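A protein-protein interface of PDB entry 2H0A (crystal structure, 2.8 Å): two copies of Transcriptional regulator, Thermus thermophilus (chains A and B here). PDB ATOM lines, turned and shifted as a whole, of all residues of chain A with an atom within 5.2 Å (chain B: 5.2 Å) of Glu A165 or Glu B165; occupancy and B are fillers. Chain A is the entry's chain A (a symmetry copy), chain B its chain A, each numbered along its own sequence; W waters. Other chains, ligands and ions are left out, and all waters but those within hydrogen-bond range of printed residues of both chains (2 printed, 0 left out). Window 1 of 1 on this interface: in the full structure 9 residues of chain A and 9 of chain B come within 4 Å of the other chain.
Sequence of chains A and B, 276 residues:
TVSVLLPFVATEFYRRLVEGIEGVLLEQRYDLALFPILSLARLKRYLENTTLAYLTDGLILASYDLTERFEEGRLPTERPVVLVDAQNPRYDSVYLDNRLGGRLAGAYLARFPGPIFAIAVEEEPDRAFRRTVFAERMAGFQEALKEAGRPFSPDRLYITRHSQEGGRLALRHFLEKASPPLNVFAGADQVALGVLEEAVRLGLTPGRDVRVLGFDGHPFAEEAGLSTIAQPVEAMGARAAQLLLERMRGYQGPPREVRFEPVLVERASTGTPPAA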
ATOM      1  N   THR A 160     -19.838  25.607  23.499  1.00  0.00           N
ATOM      2  CA  THR A 160     -21.278  25.553  23.282  1.00  0.00           C
ATOM      3  C   THR A 160     -21.766  24.129  23.000  1.00  0.00           C
ATOM      4  O   THR A 160     -21.025  23.170  23.184  1.00  0.00           O
ATOM      5  CB  THR A 160     -21.691  26.513  22.126  1.00  0.00           C
ATOM      6  OG1 THR A 160     -23.113  26.494  21.972  1.00  0.00           O
ATOM      7  CG2 THR A 160     -21.027  26.117  20.816  1.00  0.00           C
ATOM      8  N   ARG A 161     -23.016  23.995  22.566  1.00  0.00           N
ATOM      9  CA  ARG A 161     -23.592  22.683  22.282  1.00  0.00           C
ATOM     10  C   ARG A 161     -23.404  22.315  20.818  1.00  0.00           C
ATOM     11  O   ARG A 161     -23.094  23.166  19.984  1.00  0.00           O
ATOM     12  CB  ARG A 161     -25.086  22.667  22.606  1.00  0.00           C
ATOM     13  CG  ARG A 161     -25.494  23.380  23.892  1.00  0.00           C
ATOM     14  CD  ARG A 161     -25.260  22.551  25.135  1.00  0.00           C
ATOM     15  NE  ARG A 161     -25.835  21.213  25.027  1.00  0.00           N
ATOM     16  CZ  ARG A 161     -27.098  20.945  24.696  1.00  0.00           C
ATOM     17  NH1 ARG A 161     -27.944  21.932  24.432  1.00  0.00           N
ATOM     18  NH2 ARG A 161     -27.517  19.685  24.630  1.00  0.00           N
ATOM     19  N   SER A 163     -24.778  22.082  17.864  1.00  0.00           N
ATOM     20  CA  SER A 163     -25.907  22.537  17.051  1.00  0.00           C
ATOM     21  C   SER A 163     -25.494  23.694  16.161  1.00  0.00           C
ATOM     22  O   SER A 163     -24.416  24.274  16.319  1.00  0.00           O
ATOM     23  CB  SER A 163     -27.064  23.010  17.937  1.00  0.00           C
ATOM     24  OG  SER A 163     -26.736  24.213  18.620  1.00  0.00           O
ATOM     25  N   GLN A 164     -26.376  24.033  15.230  1.00  0.00           N
ATOM     26  CA  GLN A 164     -26.120  25.129  14.322  1.00  0.00           C
ATOM     27  C   GLN A 164     -26.288  26.431  15.083  1.00  0.00           C
ATOM     28  O   GLN A 164     -25.632  27.429  14.786  1.00  0.00           O
ATOM     29  CB  GLN A 164     -27.098  25.089  13.160  1.00  0.00           C
ATOM     30  CG  GLN A 164     -27.206  23.748  12.485  1.00  0.00           C
ATOM     31  CD  GLN A 164     -27.829  23.860  11.110  1.00  0.00           C
ATOM     32  OE1 GLN A 164     -28.278  22.867  10.543  1.00  0.00           O
ATOM     33  NE2 GLN A 164     -27.846  25.076  10.558  1.00  0.00           N
ATOM     34  N   GLU A 165     -27.178  26.416  16.070  1.00  0.00           N
ATOM     35  CA  GLU A 165     -27.425  27.598  16.880  1.00  0.00           C
ATOM     36  C   GLU A 165     -26.164  27.952  17.660  1.00  0.00           C
ATOM     37  O   GLU A 165     -25.840  29.130  17.810  1.00  0.00           O
ATOM     38  CB  GLU A 165     -28.591  27.360  17.844  1.00  0.00           C
ATOM     39  CG  GLU A 165     -29.942  27.184  17.164  1.00  0.00           C
ATOM     40  CD  GLU A 165     -30.104  25.827  16.507  1.00  0.00           C
ATOM     41  OE1 GLU A 165     -29.915  24.801  17.202  1.00  0.00           O
ATOM     42  OE2 GLU A 165     -30.430  25.783  15.301  1.00  0.00           O
ATOM     43  N   GLY A 166     -25.464  26.933  18.162  1.00  0.00           N
ATOM     44  CA  GLY A 166     -24.235  27.172  18.894  1.00  0.00           C
ATOM     45  C   GLY A 166     -23.208  27.851  17.998  1.00  0.00           C
ATOM     46  O   GLY A 166     -22.523  28.788  18.413  1.00  0.00           O
ATOM     47  N   GLY A 167     -23.104  27.375  16.759  1.00  0.00           N
ATOM     48  CA  GLY A 167     -22.169  27.962  15.815  1.00  0.00           C
ATOM     49  C   GLY A 167     -22.505  29.409  15.513  1.00  0.00           C
ATOM     50  O   GLY A 167     -21.620  30.250  15.373  1.00  0.00           O
ATOM     51  N   ARG A 168     -23.795  29.706  15.401  1.00  0.00           N
ATOM     52  CA  ARG A 168     -24.226  31.070  15.131  1.00  0.00           C
ATOM     53  C   ARG A 168     -23.904  31.943  16.339  1.00  0.00           C
ATOM     54  O   ARG A 168     -23.384  33.047  16.188  1.00  0.00           O
ATOM     55  CB  ARG A 168     -25.728  31.113  14.830  1.00  0.00           C
ATOM     56  CG  ARG A 168     -26.128  30.396  13.544  1.00  0.00           C
ATOM     57  CD  ARG A 168     -27.639  30.396  13.364  1.00  0.00           C
ATOM     58  NE  ARG A 168     -28.157  31.756  13.400  1.00  0.00           N
ATOM     59  CZ  ARG A 168     -29.393  32.083  13.757  1.00  0.00           C
ATOM     60  NH1 ARG A 168     -30.254  31.138  14.107  1.00  0.00           N
ATOM     61  NH2 ARG A 168     -29.760  33.363  13.782  1.00  0.00           N
ATOM     62  N   LEU A 169     -24.210  31.449  17.536  1.00  0.00           N
ATOM     63  CA  LEU A 169     -23.925  32.202  18.749  1.00  0.00           C
ATOM     64  C   LEU A 169     -22.418  32.507  18.795  1.00  0.00           C
ATOM     65  O   LEU A 169     -22.006  33.617  19.150  1.00  0.00           O
ATOM     66  CB  LEU A 169     -24.310  31.387  19.982  1.00  0.00           C
ATOM     67  CG  LEU A 169     -25.477  31.700  20.937  1.00  0.00           C
ATOM     68  CD1 LEU A 169     -26.233  32.944  20.537  1.00  0.00           C
ATOM     69  CD2 LEU A 169     -26.401  30.480  20.973  1.00  0.00           C
ATOM     70  N   ALA A 170     -21.605  31.521  18.417  1.00  0.00           N
ATOM     71  CA  ALA A 170     -20.149  31.660  18.428  1.00  0.00           C
ATOM     72  C   ALA A 170     -19.586  32.689  17.445  1.00  0.00           C
ATOM     73  O   ALA A 170     -18.790  33.535  17.826  1.00  0.00           O
ATOM     74  CB  ALA A 170     -19.498  30.301  18.191  1.00  0.00           C
ATOM     75  N   THR B 160     -37.130  28.571  16.014  1.00  0.00           N
ATOM     76  CA  THR B 160     -35.829  27.979  16.295  1.00  0.00           C
ATOM     77  C   THR B 160     -35.951  26.561  16.860  1.00  0.00           C
ATOM     78  O   THR B 160     -37.025  25.969  16.831  1.00  0.00           O
ATOM     79  CB  THR B 160     -35.015  28.887  17.266  1.00  0.00           C
ATOM     80  OG1 THR B 160     -33.719  28.321  17.478  1.00  0.00           O
ATOM     81  CG2 THR B 160     -35.730  29.050  18.598  1.00  0.00           C
ATOM     82  N   ARG B 161     -34.847  26.015  17.361  1.00  0.00           N
ATOM     83  CA  ARG B 161     -34.842  24.661  17.911  1.00  0.00           C
ATOM     84  C   ARG B 161     -35.105  24.684  19.409  1.00  0.00           C
ATOM     85  O   ARG B 161     -35.008  25.728  20.054  1.00  0.00           O
ATOM     86  CB  ARG B 161     -33.498  23.978  17.657  1.00  0.00           C
ATOM     87  CG  ARG B 161     -32.887  24.208  16.276  1.00  0.00           C
ATOM     88  CD  ARG B 161     -33.488  23.328  15.204  1.00  0.00           C
ATOM     89  NE  ARG B 161     -33.503  21.918  15.585  1.00  0.00           N
ATOM     90  CZ  ARG B 161     -32.445  21.228  16.011  1.00  0.00           C
ATOM     91  NH1 ARG B 161     -31.261  21.816  16.119  1.00  0.00           N
ATOM     92  NH2 ARG B 161     -32.572  19.943  16.330  1.00  0.00           N
ATOM     93  N   SER B 163     -33.825  24.474  22.407  1.00  0.00           N
ATOM     94  CA  SER B 163     -32.577  24.576  23.164  1.00  0.00           C
ATOM     95  C   SER B 163     -32.448  25.945  23.803  1.00  0.00           C
ATOM     96  O   SER B 163     -33.203  26.872  23.496  1.00  0.00           O
ATOM     97  CB  SER B 163     -31.364  24.362  22.253  1.00  0.00           C
ATOM     98  OG  SER B 163     -31.202  25.442  21.343  1.00  0.00           O
ATOM     99  N   GLN B 164     -31.467  26.066  24.688  1.00  0.00           N
ATOM    100  CA  GLN B 164     -31.219  27.320  25.363  1.00  0.00           C
ATOM    101  C   GLN B 164     -30.568  28.273  24.378  1.00  0.00           C
ATOM    102  O   GLN B 164     -30.749  29.488  24.455  1.00  0.00           O
ATOM    103  CB  GLN B 164     -30.295  27.107  26.550  1.00  0.00           C
ATOM    104  CG  GLN B 164     -30.714  25.991  27.470  1.00  0.00           C
ATOM    105  CD  GLN B 164     -30.045  26.097  28.823  1.00  0.00           C
ATOM    106  OE1 GLN B 164     -30.015  25.134  29.584  1.00  0.00           O
ATOM    107  NE2 GLN B 164     -29.513  27.282  29.136  1.00  0.00           N
ATOM    108  N   GLU B 165     -29.801  27.712  23.448  1.00  0.00           N
ATOM    109  CA  GLU B 165     -29.129  28.516  22.440  1.00  0.00           C
ATOM    110  C   GLU B 165     -30.167  29.198  21.557  1.00  0.00           C
ATOM    111  O   GLU B 165     -29.991  30.355  21.175  1.00  0.00           O
ATOM    112  CB  GLU B 165     -28.199  27.648  21.587  1.00  0.00           C
ATOM    113  CG  GLU B 165     -27.010  27.070  22.342  1.00  0.00           C
ATOM    114  CD  GLU B 165     -27.388  25.915  23.249  1.00  0.00           C
ATOM    115  OE1 GLU B 165     -28.005  24.944  22.752  1.00  0.00           O
ATOM    116  OE2 GLU B 165     -27.058  25.971  24.453  1.00  0.00           O
ATOM    117  N   GLY B 166     -31.240  28.477  21.229  1.00  0.00           N
ATOM    118  CA  GLY B 166     -32.295  29.052  20.415  1.00  0.00           C
ATOM    119  C   GLY B 166     -32.920  30.245  21.125  1.00  0.00           C
ATOM    120  O   GLY B 166     -33.182  31.283  20.514  1.00  0.00           O
ATOM    121  N   GLY B 167     -33.159  30.095  22.426  1.00  0.00           N
ATOM    122  CA  GLY B 167     -33.736  31.177  23.205  1.00  0.00           C
ATOM    123  C   GLY B 167     -32.829  32.392  23.242  1.00  0.00           C
ATOM    124  O   GLY B 167     -33.290  33.530  23.185  1.00  0.00           O
ATOM    125  N   ARG B 168     -31.526  32.154  23.348  1.00  0.00           N
ATOM    126  CA  ARG B 168     -30.567  33.250  23.373  1.00  0.00           C
ATOM    127  C   ARG B 168     -30.556  33.933  22.010  1.00  0.00           C
ATOM    128  O   ARG B 168     -30.576  35.160  21.930  1.00  0.00           O
ATOM    129  CB  ARG B 168     -29.167  32.735  23.722  1.00  0.00           C
ATOM    130  CG  ARG B 168     -29.041  32.174  25.134  1.00  0.00           C
ATOM    131  CD  ARG B 168     -27.654  31.593  25.371  1.00  0.00           C
ATOM    132  NE  ARG B 168     -26.631  32.592  25.101  1.00  0.00           N
ATOM    133  CZ  ARG B 168     -25.384  32.316  24.740  1.00  0.00           C
ATOM    134  NH1 ARG B 168     -24.996  31.055  24.608  1.00  0.00           N
ATOM    135  NH2 ARG B 168     -24.530  33.306  24.488  1.00  0.00           N
ATOM    136  N   LEU B 169     -30.525  33.142  20.941  1.00  0.00           N
ATOM    137  CA  LEU B 169     -30.528  33.703  19.597  1.00  0.00           C
ATOM    138  C   LEU B 169     -31.782  34.579  19.434  1.00  0.00           C
ATOM    139  O   LEU B 169     -31.722  35.672  18.860  1.00  0.00           O
ATOM    140  CB  LEU B 169     -30.558  32.585  18.556  1.00  0.00           C
ATOM    141  CG  LEU B 169     -29.404  32.211  17.608  1.00  0.00           C
ATOM    142  CD1 LEU B 169     -28.193  33.092  17.796  1.00  0.00           C
ATOM    143  CD2 LEU B 169     -29.058  30.738  17.840  1.00  0.00           C
ATOM    144  N   ALA B 170     -32.910  34.099  19.957  1.00  0.00           N
ATOM    145  CA  ALA B 170     -34.184  34.812  19.862  1.00  0.00           C
ATOM    146  C   ALA B 170     -34.240  36.146  20.610  1.00  0.00           C
ATOM    147  O   ALA B 170     -34.638  37.155  20.044  1.00  0.00           O
ATOM    148  CB  ALA B 170     -35.320  33.906  20.325  1.00  0.00           C
HETATM  149  O   HOH W   1     -32.587  29.273  15.060  1.00  0.00           O
HETATM  150  O   HOH W   2     -23.662  28.260  24.119  1.00  0.00           O
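Glu B165 touches just these residues of chain A: Thr A160, Arg A161, Glu A165 and Leu A169. Of the printed residues of chain A, Thr B160 touches Glu A165 (3.96 Å). Printed residues of chain B within 4 Å of Arg A168: Leu B169 (3.8 Å). The nearest residue of chain B that does not touch Glu A165 is Ser B163 (4.4 Å). The nearest residue of chain A that does not touch Glu B165 is Ser A163 (4.4 Å).
The backbone NH (N) of Glu B165 sits close to the side-chain hydroxyl (OG) of Ser B163. N of Glu A165 lies close to OG of Ser A163, 3.4 Å away.
Thr A160 touches Glu B165, and with the chains exchanged Glu A165 touches Thr B160. Arg A161 touches Glu B165, and with the chains exchanged Glu A165 touches Arg B161. Glu A165 touches its own counterpart, Glu B165. Glu A165 touches Leu B169, and with the chains exchanged Leu A169 touches Glu B165. Positions printed for both chains: 160, 161, 163, 164, 165, 166, 167, 168, 169 and 170.
Glu B165 touches Thr A160. Thr B160 touches Glu A165. Glu A165 touches Glu B165 (CB to CB, 3.8 Å). Glu A165 touches Leu B169. NH1 of Arg A168 touches CG of Leu B169, at 3.8 Å. CD2 of Leu A169 touches CB of Glu B165 (3.4 Å). Arg B168 touches Leu A169. Leu A169 touches Leu B169.
Water W2 bridges OG1 of Thr A160 (2.8 Å) and NH1 of Arg B168 (3.1 Å). Water W1 lies within hydrogen-bond range of OG1 of Thr B160 (2.8 Å) and NH1 of Arg A168 (3.1 Å).
OE1 of Glu A165 is in salt-bridge range of NH1 of Arg B161. The side-chain carboxylate of Glu B165 lies within salt-bridge range of the guanidinium group of Arg A161 (3.4 Å).
Of the 10 printed residues of chain B, 5 touch a printed residue of chain A. Printed residues of chain B that touch a printed residue of chain A: Thr B160, Arg B161, Glu B165, Arg B168 and Leu B169. Hydrophobic or aromatic side chains of chain B within 4 Å of the printed part of chain A: Leu B169. Along chain B the printed residues that touch a printed residue of chain A span positions 160 to 169. Hydrophobic or aromatic side chains of chain A that line the printed part of chain B: Leu A169. Among the printed residues, 10 pairs touch across the chains. Among the printed residues, Asp or Glu carboxylates within 4 Å of a Lys or Arg side-chain nitrogen of the other chain: Arg A161 with Glu B165 (3.4 Å) and Glu A165 with Arg B161 (3.4 Å).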
